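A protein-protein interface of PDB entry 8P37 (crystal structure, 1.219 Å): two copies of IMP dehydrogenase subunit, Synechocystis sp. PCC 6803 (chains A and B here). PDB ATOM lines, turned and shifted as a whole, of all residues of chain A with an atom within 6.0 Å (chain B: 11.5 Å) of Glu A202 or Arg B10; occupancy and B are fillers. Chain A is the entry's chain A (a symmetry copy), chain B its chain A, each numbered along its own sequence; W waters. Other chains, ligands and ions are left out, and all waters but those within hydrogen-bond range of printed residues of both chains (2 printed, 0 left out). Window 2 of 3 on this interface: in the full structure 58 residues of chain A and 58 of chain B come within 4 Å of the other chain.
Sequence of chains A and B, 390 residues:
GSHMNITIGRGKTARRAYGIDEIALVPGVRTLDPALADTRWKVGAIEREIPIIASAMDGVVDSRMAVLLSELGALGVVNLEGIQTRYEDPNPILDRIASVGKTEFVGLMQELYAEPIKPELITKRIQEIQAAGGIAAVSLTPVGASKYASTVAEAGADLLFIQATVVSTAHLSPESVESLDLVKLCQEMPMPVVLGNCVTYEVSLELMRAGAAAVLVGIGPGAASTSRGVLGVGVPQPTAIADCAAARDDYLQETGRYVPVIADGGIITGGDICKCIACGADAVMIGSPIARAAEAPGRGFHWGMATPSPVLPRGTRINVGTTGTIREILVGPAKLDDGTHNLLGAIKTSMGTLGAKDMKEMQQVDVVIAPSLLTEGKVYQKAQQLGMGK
O of Arg B10 sits close to O of Ala A242, 3.3 Å away. The side-chain hydroxyl of Thr A239 lies within hydrogen-bond range of the backbone carbonyl oxygen of Ile B8 (2.8 Å). The side-chain carboxylate of Asp A243 sits at hydrogen-bond distance from the backbone NH of Arg B10 (2.8 Å). The side-chain carboxylate of Glu A202 lies within salt-bridge range of the guanidinium group of Arg B10.
Printed residues of chain A that touch a printed residue of chain B: Tyr A201, Glu A202, Thr A239, Ala A242, Asp A243 and Ala A246. Along chain A the printed residues that touch a printed residue of chain B span positions 201 to 246. Printed residues of chain B that touch a printed residue of chain A: Ile B8, Gly B9, Arg B10 and Lys B12. Along chain B the printed residues that touch a printed residue of chain A span positions 8 to 12. Among the printed residues, 9 pairs touch across the chains.
Water W2 lies within hydrogen-bond range of the backbone carbonyl oxygen (O) of Ala A242 (2.7 Å), the backbone carbonyl oxygen (O) of Arg B10 (2.7 Å) and the backbone NH (N) of Ala A246 (3.4 Å). Water W1 lies within hydrogen-bond range of OD1 of Asp A243 (2.7 Å) and N of Arg B10 (3.4 Å).
Tyr A201 touches Arg B10 (CE1 to NH1, 3.5 Å). Gly B9 touches Ala A242. Ala A242 touches Lys B12 (CB to CB, 3.8 Å). CA of Gly B9 touches OD1 of Asp A243, 3.3 Å away. CB of Ala A246 touches CB of Arg B10 (3.6 Å).
No residue of chain B comes within 4 Å of Thr A200. Tyr A201 touches just one residue of chain B: Arg B10 (3.5 Å). Printed residues of chain B within 4 Å of Glu A202: Arg B10 (3.1 Å). No residue of chain B comes within 4 Å of Val A203. No residue of chain B comes within 4 Å of Ser A204. No residue of chain B comes within 4 Å of Leu A205. No residue of chain B comes within 4 Å of Glu A206. Of the printed residues of chain B, Thr A239 touches Ile B8. No residue of chain B comes within 4 Å of Ala A245. Ala A246 touches just one residue of chain B: Arg B10. Ile B6 touches none of the printed residues of chain A. Of the printed residues of chain A, Ile B8 touches Thr A239. Printed residues of chain A within 4 Å of Gly B9: Ala A242 and Asp A243. Of the printed residues of chain A, Lys B12 touches Ala A242. Thr B13 touches none of the printed residues of chain A. The nearest residue of chain B that does not touch Glu A202 is Gly B9 (10.8 Å). The nearest residue of chain A that does not touch Arg B10 is Asp A250 (5.1 Å).
No position is printed for both chains. Of the 9 pairs that touch across the chains among the printed residues, none has its exchanged pair printed and touching as well.
The side-chain carboxylate of Asp A250 sits at hydrogen-bond distance from the side-chain hydroxyl of Tyr A201. OG of Ser A204 lies within hydrogen-bond range of O of Tyr A201, at 3.1 Å.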
ATOM      1  N   THR A 200     -25.388  -6.197  11.702  1.00  0.00           N
ATOM      2  CA  THR A 200     -24.392  -5.796  10.692  1.00  0.00           C
ATOM      3  C   THR A 200     -24.866  -6.054   9.289  1.00  0.00           C
ATOM      4  O   THR A 200     -25.654  -6.974   8.995  1.00  0.00           O
ATOM      5  CB  THR A 200     -23.048  -6.493  10.927  1.00  0.00           C
ATOM      6  OG1 THR A 200     -23.166  -7.911  10.741  1.00  0.00           O
ATOM      7  CG2 THR A 200     -22.485  -6.204  12.293  1.00  0.00           C
ATOM      8  N   TYR A 201     -24.254  -5.278   8.372  1.00  0.00           N
ATOM      9  CA  TYR A 201     -24.476  -5.444   6.943  1.00  0.00           C
ATOM     10  C   TYR A 201     -24.093  -6.844   6.490  1.00  0.00           C
ATOM     11  O   TYR A 201     -24.835  -7.461   5.752  1.00  0.00           O
ATOM     12  CB  TYR A 201     -23.592  -4.409   6.218  1.00  0.00           C
ATOM     13  CG  TYR A 201     -23.587  -4.520   4.715  1.00  0.00           C
ATOM     14  CD1 TYR A 201     -22.728  -5.390   4.067  1.00  0.00           C
ATOM     15  CD2 TYR A 201     -24.533  -3.863   3.948  1.00  0.00           C
ATOM     16  CE1 TYR A 201     -22.780  -5.570   2.697  1.00  0.00           C
ATOM     17  CE2 TYR A 201     -24.545  -3.980   2.559  1.00  0.00           C
ATOM     18  CZ  TYR A 201     -23.682  -4.850   1.946  1.00  0.00           C
ATOM     19  OH  TYR A 201     -23.716  -5.024   0.576  1.00  0.00           O
ATOM     20  N   GLU A 202     -22.926  -7.337   6.923  1.00  0.00           N
ATOM     21  CA  GLU A 202     -22.421  -8.602   6.419  1.00  0.00           C
ATOM     22  C   GLU A 202     -23.320  -9.756   6.806  1.00  0.00           C
ATOM     23  O   GLU A 202     -23.616 -10.619   5.957  1.00  0.00           O
ATOM     24  CB  GLU A 202     -20.997  -8.855   6.924  1.00  0.00           C
ATOM     25  CG  GLU A 202     -19.949  -7.874   6.390  1.00  0.00           C
ATOM     26  CD  GLU A 202     -19.899  -6.442   6.914  1.00  0.00           C
ATOM     27  OE1 GLU A 202     -20.552  -6.123   7.932  1.00  0.00           O
ATOM     28  OE2 GLU A 202     -19.184  -5.626   6.288  1.00  0.00           O
ATOM     29  N   VAL A 203     -23.800  -9.793   8.048  1.00  0.00           N
ATOM     30  CA  VAL A 203     -24.647 -10.875   8.504  1.00  0.00           C
ATOM     31  C   VAL A 203     -26.039 -10.788   7.934  1.00  0.00           C
ATOM     32  O   VAL A 203     -26.562 -11.779   7.414  1.00  0.00           O
ATOM     33  CB  VAL A 203     -24.680 -10.974  10.039  1.00  0.00           C
ATOM     34  CG1 VAL A 203     -25.673 -12.015  10.504  1.00  0.00           C
ATOM     35  CG2 VAL A 203     -23.301 -11.330  10.568  1.00  0.00           C
ATOM     36  N   SER A 204     -26.633  -9.603   7.917  1.00  0.00           N
ATOM     37  CA  SER A 204     -27.953  -9.442   7.319  1.00  0.00           C
ATOM     38  C   SER A 204     -27.952  -9.872   5.849  1.00  0.00           C
ATOM     39  O   SER A 204     -28.853 -10.593   5.422  1.00  0.00           O
ATOM     40  CB  SER A 204     -28.484  -8.040   7.523  1.00  0.00           C
ATOM     41  OG  SER A 204     -27.684  -7.039   6.967  1.00  0.00           O
ATOM     42  N   LEU A 205     -26.920  -9.507   5.089  1.00  0.00           N
ATOM     43  CA  LEU A 205     -26.803  -9.930   3.712  1.00  0.00           C
ATOM     44  C   LEU A 205     -26.729 -11.448   3.584  1.00  0.00           C
ATOM     45  O   LEU A 205     -27.375 -12.047   2.697  1.00  0.00           O
ATOM     46  CB  LEU A 205     -25.605  -9.248   3.049  1.00  0.00           C
ATOM     47  CG  LEU A 205     -25.412  -9.498   1.577  1.00  0.00           C
ATOM     48  CD1 LEU A 205     -26.677  -9.087   0.741  1.00  0.00           C
ATOM     49  CD2 LEU A 205     -24.207  -8.740   1.087  1.00  0.00           C
ATOM     50  N   GLU A 206     -25.968 -12.101   4.465  1.00  0.00           N
ATOM     51  CA  GLU A 206     -25.887 -13.549   4.460  1.00  0.00           C
ATOM     52  C   GLU A 206     -27.188 -14.237   4.813  1.00  0.00           C
ATOM     53  O   GLU A 206     -27.548 -15.261   4.210  1.00  0.00           O
ATOM     54  CB  GLU A 206     -24.741 -14.027   5.372  1.00  0.00           C
ATOM     55  CG  GLU A 206     -23.355 -13.750   4.782  1.00  0.00           C
ATOM     56  CD  GLU A 206     -23.152 -14.172   3.341  1.00  0.00           C
ATOM     57  OE1 GLU A 206     -23.344 -15.378   3.059  1.00  0.00           O
ATOM     58  OE2 GLU A 206     -22.858 -13.302   2.484  1.00  0.00           O
ATOM     59  N   LEU A 207     -27.917 -13.676   5.750  1.00  0.00           N
ATOM     60  CA  LEU A 207     -29.238 -14.213   6.103  1.00  0.00           C
ATOM     61  C   LEU A 207     -30.206 -14.095   4.924  1.00  0.00           C
ATOM     62  O   LEU A 207     -30.991 -15.013   4.639  1.00  0.00           O
ATOM     63  CB  LEU A 207     -29.815 -13.576   7.364  1.00  0.00           C
ATOM     64  CG  LEU A 207     -28.984 -13.775   8.673  1.00  0.00           C
ATOM     65  CD1 LEU A 207     -29.549 -12.966   9.821  1.00  0.00           C
ATOM     66  CD2 LEU A 207     -28.820 -15.238   9.040  1.00  0.00           C
ATOM     67  N   THR A 239     -28.061   2.827  13.939  1.00  0.00           N
ATOM     68  CA  THR A 239     -26.910   2.402  13.142  1.00  0.00           C
ATOM     69  C   THR A 239     -27.106   0.963  12.642  1.00  0.00           C
ATOM     70  O   THR A 239     -26.842   0.680  11.479  1.00  0.00           O
ATOM     71  CB  THR A 239     -25.623   2.522  13.969  1.00  0.00           C
ATOM     72  OG1 THR A 239     -25.368   3.910  14.178  1.00  0.00           O
ATOM     73  CG2 THR A 239     -24.449   1.871  13.300  1.00  0.00           C
ATOM     74  N   ALA A 242     -29.780   0.934   9.854  1.00  0.00           N
ATOM     75  CA  ALA A 242     -29.292   1.501   8.594  1.00  0.00           C
ATOM     76  C   ALA A 242     -28.363   0.528   7.879  1.00  0.00           C
ATOM     77  O   ALA A 242     -28.490   0.335   6.656  1.00  0.00           O
ATOM     78  CB  ALA A 242     -28.624   2.849   8.823  1.00  0.00           C
ATOM     79  N   ASP A 243     -27.436  -0.083   8.608  1.00  0.00           N
ATOM     80  CA  ASP A 243     -26.500  -1.014   7.995  1.00  0.00           C
ATOM     81  C   ASP A 243     -27.220  -2.230   7.371  1.00  0.00           C
ATOM     82  O   ASP A 243     -26.860  -2.686   6.270  1.00  0.00           O
ATOM     83  CB  ASP A 243     -25.478  -1.501   9.002  1.00  0.00           C
ATOM     84  CG  ASP A 243     -24.412  -0.480   9.383  1.00  0.00           C
ATOM     85  OD1 ASP A 243     -24.196   0.485   8.611  1.00  0.00           O
ATOM     86  OD2 ASP A 243     -23.718  -0.695  10.394  1.00  0.00           O
ATOM     87  N   ALA A 245     -30.462  -2.289   6.441  1.00  0.00           N
ATOM     88  CA  ALA A 245     -31.287  -1.819   5.334  1.00  0.00           C
ATOM     89  C   ALA A 245     -30.428  -1.664   4.074  1.00  0.00           C
ATOM     90  O   ALA A 245     -30.937  -1.871   2.967  1.00  0.00           O
ATOM     91  CB  ALA A 245     -31.953  -0.502   5.674  1.00  0.00           C
ATOM     92  N   ALA A 246     -29.159  -1.292   4.217  1.00  0.00           N
ATOM     93  CA  ALA A 246     -28.250  -1.212   3.083  1.00  0.00           C
ATOM     94  C   ALA A 246     -28.038  -2.624   2.506  1.00  0.00           C
ATOM     95  O   ALA A 246     -28.008  -2.779   1.282  1.00  0.00           O
ATOM     96  CB  ALA A 246     -26.939  -0.588   3.498  1.00  0.00           C
ATOM     97  N   ALA A 247     -27.939  -3.650   3.358  1.00  0.00           N
ATOM     98  CA  ALA A 247     -27.846  -5.016   2.892  1.00  0.00           C
ATOM     99  C   ALA A 247     -29.115  -5.417   2.132  1.00  0.00           C
ATOM    100  O   ALA A 247     -29.025  -6.010   1.070  1.00  0.00           O
ATOM    101  CB  ALA A 247     -27.592  -5.958   4.034  1.00  0.00           C
ATOM    102  N   ASP A 250     -28.956  -3.788  -1.321  1.00  0.00           N
ATOM    103  CA  ASP A 250     -27.978  -4.451  -2.182  1.00  0.00           C
ATOM    104  C   ASP A 250     -28.476  -5.833  -2.609  1.00  0.00           C
ATOM    105  O   ASP A 250     -28.325  -6.218  -3.762  1.00  0.00           O
ATOM    106  CB  ASP A 250     -26.619  -4.524  -1.475  1.00  0.00           C
ATOM    107  CG  ASP A 250     -25.881  -3.204  -1.407  1.00  0.00           C
ATOM    108  OD1 ASP A 250     -26.307  -2.236  -2.079  1.00  0.00           O
ATOM    109  OD2 ASP A 250     -24.898  -3.113  -0.647  1.00  0.00           O
ATOM    110  N   ILE B   6     -22.613  13.390   8.717  1.00  0.00           N
ATOM    111  CA  ILE B   6     -22.507  12.294   9.691  1.00  0.00           C
ATOM    112  C   ILE B   6     -23.063  11.025   9.074  1.00  0.00           C
ATOM    113  O   ILE B   6     -24.123  11.087   8.502  1.00  0.00           O
ATOM    114  CB  ILE B   6     -23.298  12.613  11.003  1.00  0.00           C
ATOM    115  CG1 ILE B   6     -22.487  13.652  11.854  1.00  0.00           C
ATOM    116  CG2 ILE B   6     -23.540  11.338  11.847  1.00  0.00           C
ATOM    117  CD1 ILE B   6     -23.189  14.253  12.910  1.00  0.00           C
ATOM    118  N   THR B   7     -22.424   9.881   9.248  1.00  0.00           N
ATOM    119  CA  THR B   7     -22.962   8.602   8.849  1.00  0.00           C
ATOM    120  C   THR B   7     -23.647   7.935  10.051  1.00  0.00           C
ATOM    121  O   THR B   7     -22.968   7.620  11.019  1.00  0.00           O
ATOM    122  CB  THR B   7     -21.822   7.720   8.312  1.00  0.00           C
ATOM    123  OG1 THR B   7     -21.292   8.401   7.168  1.00  0.00           O
ATOM    124  CG2 THR B   7     -22.270   6.344   7.941  1.00  0.00           C
ATOM    125  N   ILE B   8     -24.936   7.694   9.983  1.00  0.00           N
ATOM    126  CA  ILE B   8     -25.628   6.865  10.986  1.00  0.00           C
ATOM    127  C   ILE B   8     -25.235   5.414  10.673  1.00  0.00           C
ATOM    128  O   ILE B   8     -24.856   4.665  11.562  1.00  0.00           O
ATOM    129  CB  ILE B   8     -27.153   7.052  10.980  1.00  0.00           C
ATOM    130  CG1 ILE B   8     -27.507   8.439  11.567  1.00  0.00           C
ATOM    131  CG2 ILE B   8     -27.818   5.931  11.825  1.00  0.00           C
ATOM    132  CD1 ILE B   8     -28.908   8.867  11.407  1.00  0.00           C
ATOM    133  N   GLY B   9     -25.353   5.005   9.427  1.00  0.00           N
ATOM    134  CA  GLY B   9     -24.935   3.706   8.952  1.00  0.00           C
ATOM    135  C   GLY B   9     -24.843   3.740   7.449  1.00  0.00           C
ATOM    136  O   GLY B   9     -25.041   4.799   6.853  1.00  0.00           O
ATOM    137  N   ARG B  10     -24.591   2.608   6.837  1.00  0.00           N
ATOM    138  CA  ARG B  10     -24.449   2.581   5.366  1.00  0.00           C
ATOM    139  C   ARG B  10     -25.734   3.092   4.699  1.00  0.00           C
ATOM    140  O   ARG B  10     -26.833   2.726   5.142  1.00  0.00           O
ATOM    141  CB  ARG B  10     -24.187   1.174   4.886  1.00  0.00           C
ATOM    142  CG  ARG B  10     -22.899   0.550   5.366  1.00  0.00           C
ATOM    143  CD  ARG B  10     -22.714  -0.695   4.543  1.00  0.00           C
ATOM    144  NE  ARG B  10     -21.601  -1.534   4.965  1.00  0.00           N
ATOM    145  CZ  ARG B  10     -20.923  -2.350   4.159  1.00  0.00           C
ATOM    146  NH1 ARG B  10     -21.248  -2.450   2.867  1.00  0.00           N
ATOM    147  NH2 ARG B  10     -19.930  -3.085   4.637  1.00  0.00           N
ATOM    148  N   GLY B  11     -25.603   4.059   3.819  1.00  0.00           N
ATOM    149  CA  GLY B  11     -26.761   4.635   3.148  1.00  0.00           C
ATOM    150  C   GLY B  11     -27.681   5.543   3.957  1.00  0.00           C
ATOM    151  O   GLY B  11     -28.790   5.847   3.492  1.00  0.00           O
ATOM    152  N   LYS B  12     -27.298   5.948   5.182  1.00  0.00           N
ATOM    153  CA  LYS B  12     -28.108   6.862   5.981  1.00  0.00           C
ATOM    154  C   LYS B  12     -27.208   7.885   6.629  1.00  0.00           C
ATOM    155  O   LYS B  12     -26.369   7.558   7.477  1.00  0.00           O
ATOM    156  CB  LYS B  12     -28.921   6.170   7.067  1.00  0.00           C
ATOM    157  CG  LYS B  12     -29.990   7.063   7.710  1.00  0.00           C
ATOM    158  CD  LYS B  12     -31.216   7.245   6.803  1.00  0.00           C
ATOM    159  CE  LYS B  12     -32.171   8.311   7.254  1.00  0.00           C
ATOM    160  NZ  LYS B  12     -33.376   8.351   6.370  1.00  0.00           N
ATOM    161  N   THR B  13     -27.380   9.134   6.240  1.00  0.00           N
ATOM    162  CA  THR B  13     -26.608  10.251   6.710  1.00  0.00           C
ATOM    163  C   THR B  13     -27.464  11.181   7.552  1.00  0.00           C
ATOM    164  O   THR B  13     -28.683  10.996   7.654  1.00  0.00           O
ATOM    165  CB  THR B  13     -25.883  10.932   5.542  1.00  0.00           C
ATOM    166  OG1 THR B  13     -26.858  11.537   4.705  1.00  0.00           O
ATOM    167  CG2 THR B  13     -24.948   9.983   4.823  1.00  0.00           C
ATOM    168  N   ALA B  14     -26.799  12.046   8.268  1.00  0.00           N
ATOM    169  CA  ALA B  14     -27.450  12.978   9.175  1.00  0.00           C
ATOM    170  C   ALA B  14     -26.572  14.183   9.371  1.00  0.00           C
ATOM    171  O   ALA B  14     -25.504  14.260   8.791  1.00  0.00           O
ATOM    172  CB  ALA B  14     -27.701  12.268  10.516  1.00  0.00           C
HETATM  173  O   HOH W   1     -21.823   1.762   8.605  1.00  0.00           O
HETATM  174  O   HOH W   2     -29.417   2.052   4.837  1.00  0.00           O
